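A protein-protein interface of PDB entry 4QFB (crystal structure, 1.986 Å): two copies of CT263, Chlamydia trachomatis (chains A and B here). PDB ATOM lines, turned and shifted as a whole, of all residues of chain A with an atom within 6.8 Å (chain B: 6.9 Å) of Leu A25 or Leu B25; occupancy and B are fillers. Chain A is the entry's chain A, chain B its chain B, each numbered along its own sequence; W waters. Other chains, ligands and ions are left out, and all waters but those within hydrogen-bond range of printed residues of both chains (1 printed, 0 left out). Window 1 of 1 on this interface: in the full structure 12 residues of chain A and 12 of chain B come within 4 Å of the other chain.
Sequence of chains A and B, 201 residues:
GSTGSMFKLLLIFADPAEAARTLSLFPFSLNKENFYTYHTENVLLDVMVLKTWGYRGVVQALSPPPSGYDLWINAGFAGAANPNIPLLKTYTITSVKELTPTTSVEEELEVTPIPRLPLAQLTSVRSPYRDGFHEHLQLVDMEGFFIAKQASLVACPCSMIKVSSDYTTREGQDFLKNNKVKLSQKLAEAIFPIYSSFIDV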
ATOM      1  N   ALA A  20      15.580 -23.397   4.533  1.00  0.00           N
ATOM      2  CA  ALA A  20      15.650 -24.793   4.107  1.00  0.00           C
ATOM      3  C   ALA A  20      14.294 -25.506   4.157  1.00  0.00           C
ATOM      4  O   ALA A  20      13.897 -26.162   3.182  1.00  0.00           O
ATOM      5  CB  ALA A  20      16.671 -25.541   4.948  1.00  0.00           C
ATOM      6  N   ARG A  21      13.586 -25.448   5.300  1.00  0.00           N
ATOM      7  CA  ARG A  21      12.371 -26.262   5.413  1.00  0.00           C
ATOM      8  C   ARG A  21      11.231 -25.694   4.575  1.00  0.00           C
ATOM      9  O   ARG A  21      10.428 -26.454   4.022  1.00  0.00           O
ATOM     10  CB  ARG A  21      11.943 -26.407   6.869  1.00  0.00           C
ATOM     11  CG  ARG A  21      12.963 -27.097   7.736  1.00  0.00           C
ATOM     12  CD  ARG A  21      13.177 -28.521   7.286  1.00  0.00           C
ATOM     13  NE  ARG A  21      11.883 -29.139   7.072  1.00  0.00           N
ATOM     14  CZ  ARG A  21      11.602 -30.026   6.130  1.00  0.00           C
ATOM     15  NH1 ARG A  21      12.548 -30.456   5.328  1.00  0.00           N
ATOM     16  NH2 ARG A  21      10.366 -30.508   6.010  1.00  0.00           N
ATOM     17  N   THR A  22      11.143 -24.372   4.453  1.00  0.00           N
ATOM     18  CA  THR A  22      10.180 -23.778   3.535  1.00  0.00           C
ATOM     19  C   THR A  22      10.464 -24.241   2.110  1.00  0.00           C
ATOM     20  O   THR A  22       9.535 -24.583   1.375  1.00  0.00           O
ATOM     21  CB  THR A  22      10.190 -22.232   3.636  1.00  0.00           C
ATOM     22  OG1 THR A  22       9.718 -21.801   4.943  1.00  0.00           O
ATOM     23  CG2 THR A  22       9.316 -21.602   2.567  1.00  0.00           C
ATOM     24  N   LEU A  23      11.739 -24.300   1.701  1.00  0.00           N
ATOM     25  CA  LEU A  23      12.031 -24.772   0.348  1.00  0.00           C
ATOM     26  C   LEU A  23      11.658 -26.233   0.142  1.00  0.00           C
ATOM     27  O   LEU A  23      11.439 -26.637  -1.006  1.00  0.00           O
ATOM     28  CB  LEU A  23      13.507 -24.558   0.010  1.00  0.00           C
ATOM     29  CG  LEU A  23      13.856 -23.064  -0.080  1.00  0.00           C
ATOM     30  CD1 LEU A  23      15.360 -22.862  -0.195  1.00  0.00           C
ATOM     31  CD2 LEU A  23      13.115 -22.362  -1.246  1.00  0.00           C
ATOM     32  N   SER A  24      11.519 -27.022   1.216  1.00  0.00           N
ATOM     33  CA  SER A  24      11.079 -28.409   1.088  1.00  0.00           C
ATOM     34  C   SER A  24       9.570 -28.552   0.959  1.00  0.00           C
ATOM     35  O   SER A  24       9.101 -29.652   0.606  1.00  0.00           O
ATOM     36  CB  SER A  24      11.539 -29.259   2.279  1.00  0.00           C
ATOM     37  OG  SER A  24      12.927 -29.421   2.228  1.00  0.00           O
ATOM     38  N   LEU A  25       8.807 -27.486   1.249  1.00  0.00           N
ATOM     39  CA  LEU A  25       7.347 -27.556   1.210  1.00  0.00           C
ATOM     40  C   LEU A  25       6.796 -27.744  -0.201  1.00  0.00           C
ATOM     41  O   LEU A  25       5.696 -28.298  -0.356  1.00  0.00           O
ATOM     42  CB  LEU A  25       6.747 -26.288   1.789  1.00  0.00           C
ATOM     43  CG  LEU A  25       6.943 -25.973   3.262  1.00  0.00           C
ATOM     44  CD1 LEU A  25       6.240 -24.677   3.573  1.00  0.00           C
ATOM     45  CD2 LEU A  25       6.396 -27.106   4.100  1.00  0.00           C
ATOM     46  N   PHE A  26       7.515 -27.269  -1.221  1.00  0.00           N
ATOM     47  CA  PHE A  26       7.043 -27.165  -2.598  1.00  0.00           C
ATOM     48  C   PHE A  26       8.136 -27.597  -3.562  1.00  0.00           C
ATOM     49  O   PHE A  26       9.330 -27.425  -3.282  1.00  0.00           O
ATOM     50  CB  PHE A  26       6.599 -25.730  -2.958  1.00  0.00           C
ATOM     51  CG  PHE A  26       5.537 -25.189  -2.065  1.00  0.00           C
ATOM     52  CD1 PHE A  26       4.222 -25.590  -2.203  1.00  0.00           C
ATOM     53  CD2 PHE A  26       5.849 -24.294  -1.069  1.00  0.00           C
ATOM     54  CE1 PHE A  26       3.250 -25.110  -1.351  1.00  0.00           C
ATOM     55  CE2 PHE A  26       4.854 -23.803  -0.241  1.00  0.00           C
ATOM     56  CZ  PHE A  26       3.571 -24.225  -0.378  1.00  0.00           C
ATOM     57  N   PRO A  27       7.748 -28.170  -4.749  1.00  0.00           N
ATOM     58  CA  PRO A  27       8.782 -28.502  -5.739  1.00  0.00           C
ATOM     59  C   PRO A  27       9.155 -27.248  -6.521  1.00  0.00           C
ATOM     60  O   PRO A  27       8.791 -27.064  -7.688  1.00  0.00           O
ATOM     61  CB  PRO A  27       8.096 -29.582  -6.584  1.00  0.00           C
ATOM     62  CG  PRO A  27       6.647 -29.189  -6.560  1.00  0.00           C
ATOM     63  CD  PRO A  27       6.403 -28.586  -5.193  1.00  0.00           C
ATOM     64  N   PHE A  28       9.855 -26.366  -5.814  1.00  0.00           N
ATOM     65  CA  PHE A  28      10.384 -25.135  -6.379  1.00  0.00           C
ATOM     66  C   PHE A  28      11.320 -25.423  -7.541  1.00  0.00           C
ATOM     67  O   PHE A  28      12.092 -26.384  -7.515  1.00  0.00           O
ATOM     68  CB  PHE A  28      11.160 -24.377  -5.312  1.00  0.00           C
ATOM     69  CG  PHE A  28      10.301 -23.654  -4.312  1.00  0.00           C
ATOM     70  CD1 PHE A  28       9.691 -22.481  -4.651  1.00  0.00           C
ATOM     71  CD2 PHE A  28      10.144 -24.134  -3.008  1.00  0.00           C
ATOM     72  CE1 PHE A  28       8.893 -21.778  -3.697  1.00  0.00           C
ATOM     73  CE2 PHE A  28       9.386 -23.442  -2.083  1.00  0.00           C
ATOM     74  CZ  PHE A  28       8.744 -22.272  -2.439  1.00  0.00           C
ATOM     75  N   TYR A  38       7.657 -21.111  -7.409  1.00  0.00           N
ATOM     76  CA  TYR A  38       6.589 -22.114  -7.489  1.00  0.00           C
ATOM     77  C   TYR A  38       5.325 -21.444  -7.999  1.00  0.00           C
ATOM     78  O   TYR A  38       4.733 -20.618  -7.292  1.00  0.00           O
ATOM     79  CB  TYR A  38       6.358 -22.741  -6.131  1.00  0.00           C
ATOM     80  CG  TYR A  38       5.318 -23.833  -6.140  1.00  0.00           C
ATOM     81  CD1 TYR A  38       5.464 -24.966  -6.939  1.00  0.00           C
ATOM     82  CD2 TYR A  38       4.221 -23.744  -5.334  1.00  0.00           C
ATOM     83  CE1 TYR A  38       4.509 -25.963  -6.916  1.00  0.00           C
ATOM     84  CE2 TYR A  38       3.273 -24.718  -5.311  1.00  0.00           C
ATOM     85  CZ  TYR A  38       3.424 -25.827  -6.083  1.00  0.00           C
ATOM     86  OH  TYR A  38       2.447 -26.794  -6.021  1.00  0.00           O
ATOM     87  N   LEU A  45       4.471 -18.150  -5.796  1.00  0.00           N
ATOM     88  CA  LEU A  45       5.250 -18.140  -4.567  1.00  0.00           C
ATOM     89  C   LEU A  45       6.721 -18.135  -4.974  1.00  0.00           C
ATOM     90  O   LEU A  45       7.220 -19.134  -5.497  1.00  0.00           O
ATOM     91  CB  LEU A  45       4.889 -19.349  -3.705  1.00  0.00           C
ATOM     92  CG  LEU A  45       5.726 -19.568  -2.457  1.00  0.00           C
ATOM     93  CD1 LEU A  45       5.596 -18.402  -1.537  1.00  0.00           C
ATOM     94  CD2 LEU A  45       5.246 -20.835  -1.795  1.00  0.00           C
ATOM     95  N   GLN A 185      11.776 -25.198  10.489  1.00  0.00           N
ATOM     96  CA  GLN A 185      10.468 -25.812  10.311  1.00  0.00           C
ATOM     97  C   GLN A 185       9.351 -24.949  10.897  1.00  0.00           C
ATOM     98  O   GLN A 185       8.232 -24.963  10.376  1.00  0.00           O
ATOM     99  CB  GLN A 185      10.460 -27.201  10.938  1.00  0.00           C
ATOM    100  CG  GLN A 185       9.124 -27.971  10.776  1.00  0.00           C
ATOM    101  CD  GLN A 185       8.836 -28.359   9.335  1.00  0.00           C
ATOM    102  OE1 GLN A 185       9.716 -28.294   8.470  1.00  0.00           O
ATOM    103  NE2 GLN A 185       7.574 -28.757   9.066  1.00  0.00           N
ATOM    104  N   LEU A 187       9.165 -21.697  10.758  1.00  0.00           N
ATOM    105  CA  LEU A 187       8.863 -20.744   9.704  1.00  0.00           C
ATOM    106  C   LEU A 187       8.047 -21.409   8.611  1.00  0.00           C
ATOM    107  O   LEU A 187       7.018 -20.869   8.179  1.00  0.00           O
ATOM    108  CB  LEU A 187      10.153 -20.162   9.139  1.00  0.00           C
ATOM    109  CG  LEU A 187      11.030 -19.352  10.111  1.00  0.00           C
ATOM    110  CD1 LEU A 187      12.296 -18.897   9.418  1.00  0.00           C
ATOM    111  CD2 LEU A 187      10.232 -18.193  10.619  1.00  0.00           C
ATOM    112  N   ALA A 188       8.462 -22.612   8.190  1.00  0.00           N
ATOM    113  CA  ALA A 188       7.714 -23.340   7.163  1.00  0.00           C
ATOM    114  C   ALA A 188       6.260 -23.567   7.566  1.00  0.00           C
ATOM    115  O   ALA A 188       5.343 -23.401   6.760  1.00  0.00           O
ATOM    116  CB  ALA A 188       8.412 -24.665   6.873  1.00  0.00           C
ATOM    117  N   GLU A 189       6.018 -23.940   8.819  1.00  0.00           N
ATOM    118  CA  GLU A 189       4.670 -24.228   9.266  1.00  0.00           C
ATOM    119  C   GLU A 189       3.838 -22.980   9.438  1.00  0.00           C
ATOM    120  O   GLU A 189       2.607 -23.073   9.461  1.00  0.00           O
ATOM    121  CB  GLU A 189       4.699 -25.052  10.572  1.00  0.00           C
ATOM    122  CG  GLU A 189       5.392 -26.379  10.364  1.00  0.00           C
ATOM    123  CD  GLU A 189       5.341 -27.305  11.576  1.00  0.00           C
ATOM    124  OE1 GLU A 189       4.811 -26.854  12.602  1.00  0.00           O
ATOM    125  OE2 GLU A 189       5.850 -28.464  11.501  1.00  0.00           O
ATOM    126  N   ILE A 191       4.252 -20.508   7.120  1.00  0.00           N
ATOM    127  CA  ILE A 191       4.089 -20.027   5.762  1.00  0.00           C
ATOM    128  C   ILE A 191       3.046 -20.863   5.004  1.00  0.00           C
ATOM    129  O   ILE A 191       2.278 -20.323   4.195  1.00  0.00           O
ATOM    130  CB  ILE A 191       5.463 -20.045   5.072  1.00  0.00           C
ATOM    131  CG1 ILE A 191       6.291 -18.853   5.588  1.00  0.00           C
ATOM    132  CG2 ILE A 191       5.334 -20.077   3.539  1.00  0.00           C
ATOM    133  CD1 ILE A 191       7.714 -18.933   5.204  1.00  0.00           C
ATOM    134  N   PHE A 192       2.960 -22.158   5.280  1.00  0.00           N
ATOM    135  CA  PHE A 192       2.054 -22.990   4.474  1.00  0.00           C
ATOM    136  C   PHE A 192       0.607 -22.535   4.626  1.00  0.00           C
ATOM    137  O   PHE A 192      -0.097 -22.425   3.605  1.00  0.00           O
ATOM    138  CB  PHE A 192       2.200 -24.487   4.798  1.00  0.00           C
ATOM    139  CG  PHE A 192       1.684 -25.371   3.667  1.00  0.00           C
ATOM    140  CD1 PHE A 192       0.329 -25.488   3.432  1.00  0.00           C
ATOM    141  CD2 PHE A 192       2.561 -26.018   2.830  1.00  0.00           C
ATOM    142  CE1 PHE A 192      -0.158 -26.267   2.382  1.00  0.00           C
ATOM    143  CE2 PHE A 192       2.088 -26.801   1.784  1.00  0.00           C
ATOM    144  CZ  PHE A 192       0.724 -26.902   1.561  1.00  0.00           C
ATOM    145  N   ALA B  20       5.949 -39.172  -1.518  1.00  0.00           N
ATOM    146  CA  ALA B  20       7.185 -38.387  -1.555  1.00  0.00           C
ATOM    147  C   ALA B  20       6.986 -36.947  -1.061  1.00  0.00           C
ATOM    148  O   ALA B  20       7.731 -36.462  -0.196  1.00  0.00           O
ATOM    149  CB  ALA B  20       7.742 -38.417  -2.976  1.00  0.00           C
ATOM    150  N   ARG B  21       5.994 -36.239  -1.606  1.00  0.00           N
ATOM    151  CA  ARG B  21       5.898 -34.815  -1.282  1.00  0.00           C
ATOM    152  C   ARG B  21       5.356 -34.592   0.132  1.00  0.00           C
ATOM    153  O   ARG B  21       5.722 -33.618   0.781  1.00  0.00           O
ATOM    154  CB  ARG B  21       5.050 -34.093  -2.325  1.00  0.00           C
ATOM    155  CG  ARG B  21       5.655 -34.105  -3.742  1.00  0.00           C
ATOM    156  CD  ARG B  21       7.012 -33.404  -3.835  1.00  0.00           C
ATOM    157  NE  ARG B  21       7.046 -32.209  -3.009  1.00  0.00           N
ATOM    158  CZ  ARG B  21       8.148 -31.566  -2.677  1.00  0.00           C
ATOM    159  NH1 ARG B  21       9.324 -31.978  -3.131  1.00  0.00           N
ATOM    160  NH2 ARG B  21       8.063 -30.484  -1.922  1.00  0.00           N
ATOM    161  N   THR B  22       4.515 -35.479   0.640  1.00  0.00           N
ATOM    162  CA  THR B  22       4.091 -35.353   2.024  1.00  0.00           C
ATOM    163  C   THR B  22       5.263 -35.560   2.959  1.00  0.00           C
ATOM    164  O   THR B  22       5.385 -34.853   3.964  1.00  0.00           O
ATOM    165  CB  THR B  22       2.981 -36.362   2.334  1.00  0.00           C
ATOM    166  OG1 THR B  22       1.805 -36.007   1.622  1.00  0.00           O
ATOM    167  CG2 THR B  22       2.646 -36.389   3.792  1.00  0.00           C
ATOM    168  N   LEU B  23       6.119 -36.557   2.657  1.00  0.00           N
ATOM    169  CA  LEU B  23       7.319 -36.798   3.462  1.00  0.00           C
ATOM    170  C   LEU B  23       8.256 -35.599   3.465  1.00  0.00           C
ATOM    171  O   LEU B  23       9.032 -35.412   4.409  1.00  0.00           O
ATOM    172  CB  LEU B  23       8.074 -38.038   2.955  1.00  0.00           C
ATOM    173  CG  LEU B  23       7.316 -39.384   3.226  1.00  0.00           C
ATOM    174  CD1 LEU B  23       8.015 -40.540   2.564  1.00  0.00           C
ATOM    175  CD2 LEU B  23       7.187 -39.618   4.739  1.00  0.00           C
ATOM    176  N   SER B  24       8.200 -34.789   2.421  1.00  0.00           N
ATOM    177  CA  SER B  24       9.006 -33.577   2.327  1.00  0.00           C
ATOM    178  C   SER B  24       8.496 -32.447   3.235  1.00  0.00           C
ATOM    179  O   SER B  24       9.256 -31.488   3.518  1.00  0.00           O
ATOM    180  CB  SER B  24       9.033 -33.146   0.870  1.00  0.00           C
ATOM    181  OG  SER B  24      10.086 -32.261   0.645  1.00  0.00           O
ATOM    182  N   LEU B  25       7.246 -32.534   3.717  1.00  0.00           N
ATOM    183  CA  LEU B  25       6.661 -31.409   4.470  1.00  0.00           C
ATOM    184  C   LEU B  25       7.250 -31.249   5.867  1.00  0.00           C
ATOM    185  O   LEU B  25       7.213 -30.141   6.427  1.00  0.00           O
ATOM    186  CB  LEU B  25       5.164 -31.586   4.607  1.00  0.00           C
ATOM    187  CG  LEU B  25       4.300 -31.607   3.343  1.00  0.00           C
ATOM    188  CD1 LEU B  25       2.851 -31.904   3.749  1.00  0.00           C
ATOM    189  CD2 LEU B  25       4.386 -30.279   2.570  1.00  0.00           C
ATOM    190  N   PHE B  26       7.753 -32.330   6.461  1.00  0.00           N
ATOM    191  CA  PHE B  26       8.171 -32.358   7.872  1.00  0.00           C
ATOM    192  C   PHE B  26       9.494 -33.095   7.992  1.00  0.00           C
ATOM    193  O   PHE B  26       9.755 -34.022   7.216  1.00  0.00           O
ATOM    194  CB  PHE B  26       7.126 -33.075   8.758  1.00  0.00           C
ATOM    195  CG  PHE B  26       5.740 -32.521   8.626  1.00  0.00           C
ATOM    196  CD1 PHE B  26       5.372 -31.364   9.305  1.00  0.00           C
ATOM    197  CD2 PHE B  26       4.814 -33.155   7.849  1.00  0.00           C
ATOM    198  CE1 PHE B  26       4.134 -30.836   9.178  1.00  0.00           C
ATOM    199  CE2 PHE B  26       3.521 -32.645   7.728  1.00  0.00           C
ATOM    200  CZ  PHE B  26       3.195 -31.469   8.376  1.00  0.00           C
ATOM    201  N   PRO B  27      10.284 -32.764   8.932  1.00  0.00           N
ATOM    202  CA  PRO B  27      11.527 -33.532   9.168  1.00  0.00           C
ATOM    203  C   PRO B  27      11.270 -34.837   9.914  1.00  0.00           C
ATOM    204  O   PRO B  27      11.591 -34.995  11.079  1.00  0.00           O
ATOM    205  CB  PRO B  27      12.356 -32.546   9.988  1.00  0.00           C
ATOM    206  CG  PRO B  27      11.321 -31.775  10.775  1.00  0.00           C
ATOM    207  CD  PRO B  27      10.145 -31.650   9.896  1.00  0.00           C
ATOM    208  N   PHE B  28      10.633 -35.784   9.228  1.00  0.00           N
ATOM    209  CA  PHE B  28      10.269 -37.054   9.831  1.00  0.00           C
ATOM    210  C   PHE B  28      11.496 -37.835  10.256  1.00  0.00           C
ATOM    211  O   PHE B  28      12.525 -37.815   9.582  1.00  0.00           O
ATOM    212  CB  PHE B  28       9.533 -37.923   8.837  1.00  0.00           C
ATOM    213  CG  PHE B  28       8.153 -37.485   8.503  1.00  0.00           C
ATOM    214  CD1 PHE B  28       7.077 -37.907   9.250  1.00  0.00           C
ATOM    215  CD2 PHE B  28       7.926 -36.719   7.384  1.00  0.00           C
ATOM    216  CE1 PHE B  28       5.785 -37.523   8.908  1.00  0.00           C
ATOM    217  CE2 PHE B  28       6.655 -36.328   7.050  1.00  0.00           C
ATOM    218  CZ  PHE B  28       5.580 -36.732   7.811  1.00  0.00           C
ATOM    219  N   TYR B  38       6.572 -38.009  12.974  1.00  0.00           N
ATOM    220  CA  TYR B  38       6.815 -36.613  13.331  1.00  0.00           C
ATOM    221  C   TYR B  38       6.012 -36.353  14.601  1.00  0.00           C
ATOM    222  O   TYR B  38       4.781 -36.284  14.570  1.00  0.00           O
ATOM    223  CB  TYR B  38       6.445 -35.667  12.185  1.00  0.00           C
ATOM    224  CG  TYR B  38       6.774 -34.210  12.410  1.00  0.00           C
ATOM    225  CD1 TYR B  38       8.041 -33.811  12.749  1.00  0.00           C
ATOM    226  CD2 TYR B  38       5.796 -33.243  12.275  1.00  0.00           C
ATOM    227  CE1 TYR B  38       8.337 -32.462  12.963  1.00  0.00           C
ATOM    228  CE2 TYR B  38       6.066 -31.919  12.497  1.00  0.00           C
ATOM    229  CZ  TYR B  38       7.331 -31.529  12.824  1.00  0.00           C
ATOM    230  OH  TYR B  38       7.590 -30.187  13.022  1.00  0.00           O
ATOM    231  N   LEU B  45       2.142 -37.342  14.032  1.00  0.00           N
ATOM    232  CA  LEU B  45       1.892 -37.569  12.615  1.00  0.00           C
ATOM    233  C   LEU B  45       2.790 -38.725  12.198  1.00  0.00           C
ATOM    234  O   LEU B  45       4.002 -38.540  12.044  1.00  0.00           O
ATOM    235  CB  LEU B  45       2.190 -36.321  11.796  1.00  0.00           C
ATOM    236  CG  LEU B  45       2.097 -36.500  10.300  1.00  0.00           C
ATOM    237  CD1 LEU B  45       0.699 -36.955   9.963  1.00  0.00           C
ATOM    238  CD2 LEU B  45       2.439 -35.175   9.631  1.00  0.00           C
ATOM    239  N   GLN B 185       2.258 -33.838  -4.872  1.00  0.00           N
ATOM    240  CA  GLN B 185       2.137 -32.533  -4.212  1.00  0.00           C
ATOM    241  C   GLN B 185       0.688 -32.173  -3.886  1.00  0.00           C
ATOM    242  O   GLN B 185       0.417 -31.503  -2.877  1.00  0.00           O
ATOM    243  CB  GLN B 185       2.770 -31.452  -5.096  1.00  0.00           C
ATOM    244  CG  GLN B 185       2.801 -30.045  -4.478  1.00  0.00           C
ATOM    245  CD  GLN B 185       3.719 -29.950  -3.281  1.00  0.00           C
ATOM    246  OE1 GLN B 185       4.639 -30.766  -3.112  1.00  0.00           O
ATOM    247  NE2 GLN B 185       3.491 -28.916  -2.439  1.00  0.00           N
ATOM    248  N   LEU B 187      -1.641 -34.186  -2.922  1.00  0.00           N
ATOM    249  CA  LEU B 187      -1.891 -34.876  -1.661  1.00  0.00           C
ATOM    250  C   LEU B 187      -1.246 -34.130  -0.495  1.00  0.00           C
ATOM    251  O   LEU B 187      -1.880 -33.916   0.547  1.00  0.00           O
ATOM    252  CB  LEU B 187      -1.366 -36.309  -1.729  1.00  0.00           C
ATOM    253  CG  LEU B 187      -2.007 -37.282  -2.762  1.00  0.00           C
ATOM    254  CD1 LEU B 187      -1.276 -38.606  -2.820  1.00  0.00           C
ATOM    255  CD2 LEU B 187      -3.450 -37.544  -2.479  1.00  0.00           C
ATOM    256  N   ALA B 188       0.015 -33.706  -0.661  1.00  0.00           N
ATOM    257  CA  ALA B 188       0.690 -32.976   0.410  1.00  0.00           C
ATOM    258  C   ALA B 188      -0.069 -31.701   0.764  1.00  0.00           C
ATOM    259  O   ALA B 188      -0.238 -31.365   1.940  1.00  0.00           O
ATOM    260  CB  ALA B 188       2.111 -32.634  -0.018  1.00  0.00           C
ATOM    261  N   GLU B 189      -0.517 -30.965  -0.245  1.00  0.00           N
ATOM    262  CA  GLU B 189      -1.189 -29.700   0.007  1.00  0.00           C
ATOM    263  C   GLU B 189      -2.561 -29.875   0.644  1.00  0.00           C
ATOM    264  O   GLU B 189      -3.090 -28.914   1.217  1.00  0.00           O
ATOM    265  CB  GLU B 189      -1.300 -28.898  -1.308  1.00  0.00           C
ATOM    266  CG  GLU B 189       0.068 -28.412  -1.758  1.00  0.00           C
ATOM    267  CD  GLU B 189       0.095 -27.617  -3.041  1.00  0.00           C
ATOM    268  OE1 GLU B 189      -0.985 -27.281  -3.564  1.00  0.00           O
ATOM    269  OE2 GLU B 189       1.216 -27.310  -3.505  1.00  0.00           O
ATOM    270  N   ALA B 190      -3.163 -31.046   0.531  1.00  0.00           N
ATOM    271  CA  ALA B 190      -4.410 -31.326   1.240  1.00  0.00           C
ATOM    272  C   ALA B 190      -4.181 -31.810   2.664  1.00  0.00           C
ATOM    273  O   ALA B 190      -5.067 -31.671   3.519  1.00  0.00           O
ATOM    274  CB  ALA B 190      -5.213 -32.395   0.485  1.00  0.00           C
ATOM    275  N   ILE B 191      -3.032 -32.413   2.923  1.00  0.00           N
ATOM    276  CA  ILE B 191      -2.741 -32.977   4.240  1.00  0.00           C
ATOM    277  C   ILE B 191      -2.258 -31.901   5.208  1.00  0.00           C
ATOM    278  O   ILE B 191      -2.583 -31.929   6.402  1.00  0.00           O
ATOM    279  CB  ILE B 191      -1.686 -34.083   4.097  1.00  0.00           C
ATOM    280  CG1 ILE B 191      -2.357 -35.326   3.539  1.00  0.00           C
ATOM    281  CG2 ILE B 191      -1.000 -34.397   5.445  1.00  0.00           C
ATOM    282  CD1 ILE B 191      -1.360 -36.372   2.996  1.00  0.00           C
ATOM    283  N   PHE B 192      -1.431 -30.979   4.727  1.00  0.00           N
ATOM    284  CA  PHE B 192      -0.837 -30.012   5.644  1.00  0.00           C
ATOM    285  C   PHE B 192      -1.890 -29.203   6.389  1.00  0.00           C
ATOM    286  O   PHE B 192      -1.735 -29.030   7.608  1.00  0.00           O
ATOM    287  CB  PHE B 192       0.144 -29.083   4.919  1.00  0.00           C
ATOM    288  CG  PHE B 192       0.987 -28.307   5.878  1.00  0.00           C
ATOM    289  CD1 PHE B 192       0.450 -27.248   6.588  1.00  0.00           C
ATOM    290  CD2 PHE B 192       2.275 -28.664   6.117  1.00  0.00           C
ATOM    291  CE1 PHE B 192       1.220 -26.535   7.499  1.00  0.00           C
ATOM    292  CE2 PHE B 192       3.031 -27.985   7.034  1.00  0.00           C
ATOM    293  CZ  PHE B 192       2.496 -26.920   7.735  1.00  0.00           C
HETATM  294  O   HOH W   1      10.851 -29.624  -2.452  1.00  0.00           O
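Arg A21 touches Pro B27 (NH2 to N, 3.7 Å). Arg B21 touches Leu A25 (NH2 to C, 3.5 Å). Leu A25 touches Leu B25 (O to CD2, 3.8 Å). Phe A26 touches Glu B189. Arg B21 touches Pro A27 (NH2 to N, 3.7 Å). Gln B185 touches Tyr A38. NE2 of Gln A185 touches CD1 of Phe B26 (3.4 Å). Gln A185 touches Tyr B38. Glu A189 touches Phe B192 (CA to CZ, 3.8 Å). Glu B189 touches Phe A192 (CG to CZ, 3.7 Å).
Ser B24 touches its own counterpart, Ser A24. Leu A25 touches Gln B185, and with the chains exchanged Gln A185 touches Leu B25. Phe A26 touches Gln B185, and with the chains exchanged Gln A185 touches Phe B26. Phe B192 touches its own counterpart, Phe A192.
Of chain B, only Arg B21 (3.5 Å), Leu B25 (3.8 Å) and Gln B185 (3.1 Å) come within 4 Å of Leu A25. Leu B25 touches three residues of chain A. Printed residues of chain B within 4 Å of Pro A27: Arg B21 (3.7 Å) and Gln B185 (3.5 Å). Of the printed residues of chain A, Phe B192 touches Glu A189 (3.8 Å) and Phe A192 (3.5 Å). Printed residues of chain B within 4 Å of Ser A24: Arg B21 and Ser B24. Of the printed residues of chain B, Phe A26 touches Arg B21, Gln B185 and Glu B189. Of the printed residues of chain A, Glu B189 touches Phe A26 (3.7 Å), Tyr A38 (2.8 Å) and Phe A192 (3.7 Å). The nearest residue of chain A that does not touch Leu B25 is Phe A192 (4.2 Å). The nearest printed residue of chain B that does not touch Arg A21 is Leu B23 (5.3 Å).
Water W1 lies within hydrogen-bond range of the backbone carbonyl oxygen (O) of Phe A26 (2.8 Å), the guanidinium group (NH1) of Arg B21 (2.9 Å) and the backbone carbonyl oxygen (O) of Leu A23 (3.4 Å).
OH of Tyr B38 sits at hydrogen-bond distance from OE2 of Glu A189 (2.9 Å). The guanidinium group (NH2) of Arg A21 sits at hydrogen-bond distance from the backbone carbonyl oxygen (O) of Ser B24 (2.9 Å). The side-chain hydroxyl (OH) of Tyr A38 lies within hydrogen-bond range of the side-chain carboxylate (OE2) of Glu B189 (2.8 Å). NH2 of Arg A21 sits close to N of Phe B26. O of Leu B25 sits at hydrogen-bond distance from NE2 of Gln A185. The side-chain amide nitrogen (NE2) of Gln B185 is in hydrogen-bond range of the backbone carbonyl oxygen (O) of Leu A25 (3.1 Å). NH2 of Arg B21 sits close to N of Phe A26. O of Ser A24 is in hydrogen-bond range of OG of Ser B24 (2.8 Å). The guanidinium group (NH2) of Arg A21 sits at hydrogen-bond distance from the backbone carbonyl oxygen (O) of Leu B25, at 3.2 Å. The guanidinium group (NH2) of Arg B21 sits at hydrogen-bond distance from the backbone carbonyl oxygen (O) of Ser A24, at 2.9 Å.
N of Tyr A38 sits at hydrogen-bond distance from O of Leu A45, at 2.8 Å. OE1 of Gln B185 is in hydrogen-bond range of NE of Arg B21 (2.8 Å). NE2 of Gln A185 is in hydrogen-bond range of OE2 of Glu A189, 3.0 Å away. The guanidinium group (NE) of Arg A21 sits at hydrogen-bond distance from the side-chain amide oxygen (OE1) of Gln A185, at 2.7 Å. The guanidinium group (NH1) of Arg A21 is in hydrogen-bond range of the side-chain hydroxyl (OG) of Ser A24 (3.3 Å). The backbone NH (N) of Tyr B38 sits at hydrogen-bond distance from the backbone carbonyl oxygen (O) of Leu B45 (2.8 Å).
Of the 17 printed residues of chain A, 9 touch a printed residue of chain B.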
